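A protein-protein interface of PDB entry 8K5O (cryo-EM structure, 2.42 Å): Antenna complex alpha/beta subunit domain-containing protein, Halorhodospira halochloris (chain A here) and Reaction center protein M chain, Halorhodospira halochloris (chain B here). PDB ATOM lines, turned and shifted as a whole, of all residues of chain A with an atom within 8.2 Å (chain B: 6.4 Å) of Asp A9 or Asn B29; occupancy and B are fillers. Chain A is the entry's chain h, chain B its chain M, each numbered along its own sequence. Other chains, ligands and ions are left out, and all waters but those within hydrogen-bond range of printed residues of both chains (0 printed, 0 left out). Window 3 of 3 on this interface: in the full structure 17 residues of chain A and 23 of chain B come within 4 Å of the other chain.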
ATOM      1  N   LEU A   4      -0.082   6.405   2.389  1.00  0.00           N
ATOM      2  CA  LEU A   4      -0.587   5.403   3.323  1.00  0.00           C
ATOM      3  C   LEU A   4       0.520   4.490   3.812  1.00  0.00           C
ATOM      4  O   LEU A   4       0.448   3.960   4.925  1.00  0.00           O
ATOM      5  CB  LEU A   4      -1.694   4.584   2.662  1.00  0.00           C
ATOM      6  CG  LEU A   4      -2.466   3.654   3.596  1.00  0.00           C
ATOM      7  CD1 LEU A   4      -3.473   4.436   4.411  1.00  0.00           C
ATOM      8  CD2 LEU A   4      -3.141   2.555   2.811  1.00  0.00           C
ATOM      9  N   TRP A   5       1.551   4.306   3.002  1.00  0.00           N
ATOM     10  CA  TRP A   5       2.667   3.452   3.360  1.00  0.00           C
ATOM     11  C   TRP A   5       3.652   4.140   4.286  1.00  0.00           C
ATOM     12  O   TRP A   5       4.588   3.493   4.762  1.00  0.00           O
ATOM     13  CB  TRP A   5       3.335   2.975   2.078  1.00  0.00           C
ATOM     14  CG  TRP A   5       2.312   2.731   1.022  1.00  0.00           C
ATOM     15  CD1 TRP A   5       2.228   3.335  -0.193  1.00  0.00           C
ATOM     16  CD2 TRP A   5       1.190   1.842   1.106  1.00  0.00           C
ATOM     17  NE1 TRP A   5       1.141   2.863  -0.884  1.00  0.00           N
ATOM     18  CE2 TRP A   5       0.487   1.947  -0.106  1.00  0.00           C
ATOM     19  CE3 TRP A   5       0.717   0.965   2.088  1.00  0.00           C
ATOM     20  CZ2 TRP A   5      -0.657   1.205  -0.366  1.00  0.00           C
ATOM     21  CZ3 TRP A   5      -0.419   0.232   1.827  1.00  0.00           C
ATOM     22  CH2 TRP A   5      -1.094   0.356   0.609  1.00  0.00           C
ATOM     23  N   LYS A   6       3.456   5.428   4.557  1.00  0.00           N
ATOM     24  CA  LYS A   6       4.133   6.077   5.667  1.00  0.00           C
ATOM     25  C   LYS A   6       3.564   5.652   7.010  1.00  0.00           C
ATOM     26  O   LYS A   6       4.241   5.807   8.032  1.00  0.00           O
ATOM     27  CB  LYS A   6       4.018   7.595   5.533  1.00  0.00           C
ATOM     28  CG  LYS A   6       4.780   8.188   4.372  1.00  0.00           C
ATOM     29  CD  LYS A   6       4.510   9.675   4.273  1.00  0.00           C
ATOM     30  CE  LYS A   6       5.154  10.419   5.428  1.00  0.00           C
ATOM     31  NZ  LYS A   6       5.017  11.894   5.295  1.00  0.00           N
ATOM     32  N   PHE A   7       2.345   5.119   7.029  1.00  0.00           N
ATOM     33  CA  PHE A   7       1.643   4.801   8.262  1.00  0.00           C
ATOM     34  C   PHE A   7       1.026   3.419   8.288  1.00  0.00           C
ATOM     35  O   PHE A   7       0.731   2.922   9.380  1.00  0.00           O
ATOM     36  CB  PHE A   7       0.537   5.831   8.526  1.00  0.00           C
ATOM     37  CG  PHE A   7       0.946   7.236   8.234  1.00  0.00           C
ATOM     38  CD1 PHE A   7       1.670   7.960   9.163  1.00  0.00           C
ATOM     39  CD2 PHE A   7       0.617   7.833   7.032  1.00  0.00           C
ATOM     40  CE1 PHE A   7       2.052   9.249   8.901  1.00  0.00           C
ATOM     41  CE2 PHE A   7       0.998   9.125   6.767  1.00  0.00           C
ATOM     42  CZ  PHE A   7       1.717   9.832   7.702  1.00  0.00           C
ATOM     43  N   VAL A   8       0.800   2.791   7.141  1.00  0.00           N
ATOM     44  CA  VAL A   8       0.274   1.436   7.075  1.00  0.00           C
ATOM     45  C   VAL A   8       1.329   0.561   6.421  1.00  0.00           C
ATOM     46  O   VAL A   8       1.863   0.910   5.364  1.00  0.00           O
ATOM     47  CB  VAL A   8      -1.059   1.375   6.307  1.00  0.00           C
ATOM     48  CG1 VAL A   8      -1.531  -0.052   6.193  1.00  0.00           C
ATOM     49  CG2 VAL A   8      -2.108   2.208   7.016  1.00  0.00           C
ATOM     50  N   ASP A   9       1.643  -0.561   7.062  1.00  0.00           N
ATOM     51  CA  ASP A   9       2.633  -1.479   6.518  1.00  0.00           C
ATOM     52  C   ASP A   9       2.100  -2.094   5.232  1.00  0.00           C
ATOM     53  O   ASP A   9       1.112  -2.835   5.251  1.00  0.00           O
ATOM     54  CB  ASP A   9       2.971  -2.559   7.540  1.00  0.00           C
ATOM     55  CG  ASP A   9       3.805  -3.670   6.955  1.00  0.00           C
ATOM     56  OD1 ASP A   9       4.862  -3.374   6.366  1.00  0.00           O
ATOM     57  OD2 ASP A   9       3.416  -4.845   7.098  1.00  0.00           O
ATOM     58  N   PHE A  10       2.754  -1.783   4.111  1.00  0.00           N
ATOM     59  CA  PHE A  10       2.266  -2.259   2.824  1.00  0.00           C
ATOM     60  C   PHE A  10       2.395  -3.765   2.696  1.00  0.00           C
ATOM     61  O   PHE A  10       1.585  -4.391   2.012  1.00  0.00           O
ATOM     62  CB  PHE A  10       3.012  -1.592   1.675  1.00  0.00           C
ATOM     63  CG  PHE A  10       2.769  -2.246   0.350  1.00  0.00           C
ATOM     64  CD1 PHE A  10       1.535  -2.153  -0.267  1.00  0.00           C
ATOM     65  CD2 PHE A  10       3.768  -2.971  -0.272  1.00  0.00           C
ATOM     66  CE1 PHE A  10       1.308  -2.758  -1.484  1.00  0.00           C
ATOM     67  CE2 PHE A  10       3.545  -3.578  -1.485  1.00  0.00           C
ATOM     68  CZ  PHE A  10       2.315  -3.470  -2.092  1.00  0.00           C
ATOM     69  N   ARG A  11       3.415  -4.359   3.311  1.00  0.00           N
ATOM     70  CA  ARG A  11       3.554  -5.807   3.253  1.00  0.00           C
ATOM     71  C   ARG A  11       2.337  -6.485   3.867  1.00  0.00           C
ATOM     72  O   ARG A  11       1.740  -7.385   3.261  1.00  0.00           O
ATOM     73  CB  ARG A  11       4.840  -6.236   3.955  1.00  0.00           C
ATOM     74  CG  ARG A  11       5.168  -7.696   3.791  1.00  0.00           C
ATOM     75  CD  ARG A  11       6.438  -8.068   4.530  1.00  0.00           C
ATOM     76  NE  ARG A  11       7.628  -7.432   3.981  1.00  0.00           N
ATOM     77  CZ  ARG A  11       8.832  -7.513   4.528  1.00  0.00           C
ATOM     78  NH1 ARG A  11       9.048  -8.221   5.622  1.00  0.00           N
ATOM     79  NH2 ARG A  11       9.844  -6.867   3.961  1.00  0.00           N
ATOM     80  N   MET A  12       1.926  -6.034   5.054  1.00  0.00           N
ATOM     81  CA  MET A  12       0.709  -6.561   5.659  1.00  0.00           C
ATOM     82  C   MET A  12      -0.494  -6.333   4.760  1.00  0.00           C
ATOM     83  O   MET A  12      -1.299  -7.237   4.550  1.00  0.00           O
ATOM     84  CB  MET A  12       0.437  -5.922   7.017  1.00  0.00           C
ATOM     85  CG  MET A  12      -0.947  -6.313   7.505  1.00  0.00           C
ATOM     86  SD  MET A  12      -1.606  -5.446   8.920  1.00  0.00           S
ATOM     87  CE  MET A  12      -3.282  -6.059   8.923  1.00  0.00           C
ATOM     88  N   THR A  13      -0.639  -5.119   4.230  1.00  0.00           N
ATOM     89  CA  THR A  13      -1.829  -4.793   3.454  1.00  0.00           C
ATOM     90  C   THR A  13      -1.926  -5.656   2.203  1.00  0.00           C
ATOM     91  O   THR A  13      -2.970  -6.248   1.926  1.00  0.00           O
ATOM     92  CB  THR A  13      -1.828  -3.309   3.089  1.00  0.00           C
ATOM     93  OG1 THR A  13      -1.777  -2.528   4.284  1.00  0.00           O
ATOM     94  CG2 THR A  13      -3.079  -2.948   2.314  1.00  0.00           C
ATOM     95  N   ALA A  14      -0.832  -5.764   1.452  1.00  0.00           N
ATOM     96  CA  ALA A  14      -0.851  -6.537   0.217  1.00  0.00           C
ATOM     97  C   ALA A  14      -1.040  -8.023   0.495  1.00  0.00           C
ATOM     98  O   ALA A  14      -1.867  -8.681  -0.147  1.00  0.00           O
ATOM     99  CB  ALA A  14       0.434  -6.293  -0.571  1.00  0.00           C
ATOM    100  N   VAL A  15      -0.293  -8.574   1.453  1.00  0.00           N
ATOM    101  CA  VAL A  15      -0.411 -10.000   1.721  1.00  0.00           C
ATOM    102  C   VAL A  15      -1.780 -10.323   2.304  1.00  0.00           C
ATOM    103  O   VAL A  15      -2.378 -11.353   1.978  1.00  0.00           O
ATOM    104  CB  VAL A  15       0.731 -10.464   2.641  1.00  0.00           C
ATOM    105  CG1 VAL A  15       0.550 -11.917   3.006  1.00  0.00           C
ATOM    106  CG2 VAL A  15       2.068 -10.243   1.961  1.00  0.00           C
ATOM    107  N   GLY A  16      -2.300  -9.454   3.169  1.00  0.00           N
ATOM    108  CA  GLY A  16      -3.613  -9.678   3.735  1.00  0.00           C
ATOM    109  C   GLY A  16      -4.720  -9.545   2.714  1.00  0.00           C
ATOM    110  O   GLY A  16      -5.698 -10.288   2.754  1.00  0.00           O
ATOM    111  N   PRO B  24      10.942  -8.674  11.997  1.00  0.00           N
ATOM    112  CA  PRO B  24      10.629  -7.881  10.798  1.00  0.00           C
ATOM    113  C   PRO B  24       9.149  -7.536  10.740  1.00  0.00           C
ATOM    114  O   PRO B  24       8.284  -8.415  10.746  1.00  0.00           O
ATOM    115  CB  PRO B  24      11.061  -8.795   9.648  1.00  0.00           C
ATOM    116  CG  PRO B  24      11.014 -10.164  10.208  1.00  0.00           C
ATOM    117  CD  PRO B  24      11.394 -10.033  11.653  1.00  0.00           C
ATOM    118  N   GLY B  25       8.863  -6.236  10.696  1.00  0.00           N
ATOM    119  CA  GLY B  25       7.502  -5.751  10.749  1.00  0.00           C
ATOM    120  C   GLY B  25       6.905  -5.676  12.133  1.00  0.00           C
ATOM    121  O   GLY B  25       5.723  -5.344  12.264  1.00  0.00           O
ATOM    122  N   GLY B  26       7.685  -5.972  13.173  1.00  0.00           N
ATOM    123  CA  GLY B  26       7.145  -5.987  14.520  1.00  0.00           C
ATOM    124  C   GLY B  26       6.747  -4.623  15.039  1.00  0.00           C
ATOM    125  O   GLY B  26       5.743  -4.497  15.744  1.00  0.00           O
ATOM    126  N   SER B  27       7.521  -3.587  14.711  1.00  0.00           N
ATOM    127  CA  SER B  27       7.216  -2.256  15.223  1.00  0.00           C
ATOM    128  C   SER B  27       5.831  -1.807  14.784  1.00  0.00           C
ATOM    129  O   SER B  27       5.095  -1.185  15.559  1.00  0.00           O
ATOM    130  CB  SER B  27       8.272  -1.256  14.762  1.00  0.00           C
ATOM    131  OG  SER B  27       8.073   0.007  15.371  1.00  0.00           O
ATOM    132  N   TRP B  28       5.453  -2.120  13.548  1.00  0.00           N
ATOM    133  CA  TRP B  28       4.134  -1.732  13.077  1.00  0.00           C
ATOM    134  C   TRP B  28       3.081  -2.765  13.458  1.00  0.00           C
ATOM    135  O   TRP B  28       2.039  -2.413  14.014  1.00  0.00           O
ATOM    136  CB  TRP B  28       4.164  -1.518  11.566  1.00  0.00           C
ATOM    137  CG  TRP B  28       2.973  -0.799  11.046  1.00  0.00           C
ATOM    138  CD1 TRP B  28       2.838   0.545  10.884  1.00  0.00           C
ATOM    139  CD2 TRP B  28       1.736  -1.379  10.630  1.00  0.00           C
ATOM    140  NE1 TRP B  28       1.595   0.841  10.388  1.00  0.00           N
ATOM    141  CE2 TRP B  28       0.898  -0.326  10.223  1.00  0.00           C
ATOM    142  CE3 TRP B  28       1.256  -2.687  10.559  1.00  0.00           C
ATOM    143  CZ2 TRP B  28      -0.388  -0.541   9.746  1.00  0.00           C
ATOM    144  CZ3 TRP B  28      -0.015  -2.894  10.095  1.00  0.00           C
ATOM    145  CH2 TRP B  28      -0.827  -1.831   9.693  1.00  0.00           C
ATOM    146  N   ASN B  29       3.349  -4.045  13.208  1.00  0.00           N
ATOM    147  CA  ASN B  29       2.317  -5.063  13.359  1.00  0.00           C
ATOM    148  C   ASN B  29       2.048  -5.464  14.803  1.00  0.00           C
ATOM    149  O   ASN B  29       1.065  -6.162  15.050  1.00  0.00           O
ATOM    150  CB  ASN B  29       2.680  -6.307  12.553  1.00  0.00           C
ATOM    151  CG  ASN B  29       2.605  -6.077  11.064  1.00  0.00           C
ATOM    152  OD1 ASN B  29       1.620  -6.429  10.424  1.00  0.00           O
ATOM    153  ND2 ASN B  29       3.650  -5.486  10.502  1.00  0.00           N
ATOM    154  N   ARG B  30       2.879  -5.069  15.760  1.00  0.00           N
ATOM    155  CA  ARG B  30       2.580  -5.358  17.159  1.00  0.00           C
ATOM    156  C   ARG B  30       1.647  -4.277  17.682  1.00  0.00           C
ATOM    157  O   ARG B  30       2.031  -3.108  17.783  1.00  0.00           O
ATOM    158  CB  ARG B  30       3.855  -5.440  17.988  1.00  0.00           C
ATOM    159  CG  ARG B  30       4.399  -6.838  18.099  1.00  0.00           C
ATOM    160  CD  ARG B  30       5.770  -6.843  18.720  1.00  0.00           C
ATOM    161  NE  ARG B  30       6.381  -8.160  18.622  1.00  0.00           N
ATOM    162  CZ  ARG B  30       7.676  -8.369  18.438  1.00  0.00           C
ATOM    163  NH1 ARG B  30       8.531  -7.365  18.357  1.00  0.00           N
ATOM    164  NH2 ARG B  30       8.122  -9.617  18.336  1.00  0.00           N
ATOM    165  N   VAL B  31       0.419  -4.664  18.017  1.00  0.00           N
ATOM    166  CA  VAL B  31      -0.631  -3.709  18.332  1.00  0.00           C
ATOM    167  C   VAL B  31      -1.200  -4.015  19.707  1.00  0.00           C
ATOM    168  O   VAL B  31      -1.199  -5.156  20.173  1.00  0.00           O
ATOM    169  CB  VAL B  31      -1.752  -3.715  17.272  1.00  0.00           C
ATOM    170  CG1 VAL B  31      -1.179  -3.398  15.911  1.00  0.00           C
ATOM    171  CG2 VAL B  31      -2.463  -5.054  17.254  1.00  0.00           C
ATOM    172  N   ILE B  51      -0.310  -7.883  20.532  1.00  0.00           N
ATOM    173  CA  ILE B  51      -0.483  -8.975  19.585  1.00  0.00           C
ATOM    174  C   ILE B  51       0.064  -8.530  18.239  1.00  0.00           C
ATOM    175  O   ILE B  51       0.029  -7.346  17.888  1.00  0.00           O
ATOM    176  CB  ILE B  51      -1.962  -9.411  19.487  1.00  0.00           C
ATOM    177  CG1 ILE B  51      -2.078 -10.790  18.839  1.00  0.00           C
ATOM    178  CG2 ILE B  51      -2.783  -8.391  18.726  1.00  0.00           C
ATOM    179  CD1 ILE B  51      -3.429 -11.425  19.018  1.00  0.00           C
ATOM    180  N   TYR B  52       0.613  -9.481  17.490  1.00  0.00           N
ATOM    181  CA  TYR B  52       1.118  -9.195  16.155  1.00  0.00           C
ATOM    182  C   TYR B  52      -0.046  -9.123  15.178  1.00  0.00           C
ATOM    183  O   TYR B  52      -0.817 -10.077  15.048  1.00  0.00           O
ATOM    184  CB  TYR B  52       2.123 -10.251  15.712  1.00  0.00           C
ATOM    185  CG  TYR B  52       2.941  -9.852  14.514  1.00  0.00           C
ATOM    186  CD1 TYR B  52       4.105  -9.113  14.657  1.00  0.00           C
ATOM    187  CD2 TYR B  52       2.550 -10.218  13.235  1.00  0.00           C
ATOM    188  CE1 TYR B  52       4.857  -8.754  13.561  1.00  0.00           C
ATOM    189  CE2 TYR B  52       3.291  -9.861  12.137  1.00  0.00           C
ATOM    190  CZ  TYR B  52       4.444  -9.132  12.302  1.00  0.00           C
ATOM    191  OH  TYR B  52       5.177  -8.777  11.196  1.00  0.00           O
ATOM    192  N   LEU B  53      -0.169  -7.988  14.501  1.00  0.00           N
ATOM    193  CA  LEU B  53      -1.268  -7.729  13.577  1.00  0.00           C
ATOM    194  C   LEU B  53      -0.851  -8.086  12.150  1.00  0.00           C
ATOM    195  O   LEU B  53      -0.941  -7.284  11.226  1.00  0.00           O
ATOM    196  CB  LEU B  53      -1.683  -6.266  13.677  1.00  0.00           C
ATOM    197  CG  LEU B  53      -3.019  -5.791  13.133  1.00  0.00           C
ATOM    198  CD1 LEU B  53      -4.129  -6.172  14.094  1.00  0.00           C
ATOM    199  CD2 LEU B  53      -2.977  -4.300  12.875  1.00  0.00           C
ATOM    200  N   GLY B  54      -0.376  -9.308  11.980  1.00  0.00           N
ATOM    201  CA  GLY B  54       0.145  -9.712  10.694  1.00  0.00           C
ATOM    202  C   GLY B  54      -0.938  -9.901   9.657  1.00  0.00           C
ATOM    203  O   GLY B  54      -2.130  -9.900   9.953  1.00  0.00           O
ATOM    204  N   ALA B  55      -0.504 -10.056   8.407  1.00  0.00           N
ATOM    205  CA  ALA B  55      -1.454 -10.306   7.329  1.00  0.00           C
ATOM    206  C   ALA B  55      -2.178 -11.629   7.534  1.00  0.00           C
ATOM    207  O   ALA B  55      -3.411 -11.688   7.494  1.00  0.00           O
ATOM    208  CB  ALA B  55      -0.734 -10.288   5.982  1.00  0.00           C
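Among the printed residues, pairs that only touch across the chains: Val A8 with Trp B28 (3.4 Å), Asp A9 with Trp B28 (3.3 Å), Met A12 with Trp B28 (3.2 Å), Met A12 with Ala B55 (3.4 Å), Val A15 with Ala B55 (3.6 Å) and Gly A16 with Ala B55 (3.3 Å).
The side-chain amide oxygen (OD1) of Asn B29 lies close to the side-chain sulfur (SD) of Met A12.
NE1 of Trp B28 lies within hydrogen-bond range of O of Phe A7, at 2.5 Å.
The side-chain amide nitrogen (ND2) of Asn B29 sits at hydrogen-bond distance from the side-chain carboxylate (OD2) of Asp A9, at 3.5 Å.
O of Leu B53 lies close to SD of Met A12 (3.0 Å).
Asn B29 touches just these residues of chain A: Asp A9 and Met A12.
Printed residues of chain B within 4 Å of Gly A16: Ala B55 (3.3 Å).
Of the printed residues of chain B, Val A15 touches Ala B55 (3.6 Å).
Of the printed residues of chain A, Ala B55 touches Met A12, Val A15 and Gly A16.
Thr A13 touches none of the printed residues of chain B.
Ser B27 touches none of the printed residues of chain A.
The nearest residue of chain B that does not touch Asp A9 is Gly B25 (5.6 Å).
The nearest residue of chain A that does not touch Asn B29 is Arg A11 (6.6 Å).
OD2 of Asp A9 is in hydrogen-bond range of N of Met A12 (2.8 Å).
OD1 of Asn B29 lies close to O of Leu B53, 2.8 Å away.
The backbone carbonyl oxygen of Gly B25 lies within hydrogen-bond range of the side-chain amide nitrogen of Asn B29.
The backbone carbonyl oxygen (O) of Asp A9 lies within hydrogen-bond range of the side-chain hydroxyl (OG1) of Thr A13 (3.1 Å).
Printed residues of chain B that touch a printed residue of chain A: Trp B28, Asn B29, Leu B53 and Ala B55.
Among the printed residues, 10 pairs touch across the chains.
Among the printed residues, no Asp or Glu carboxylate lies within 4 Å of a Lys or Arg side-chain nitrogen of the other chain.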
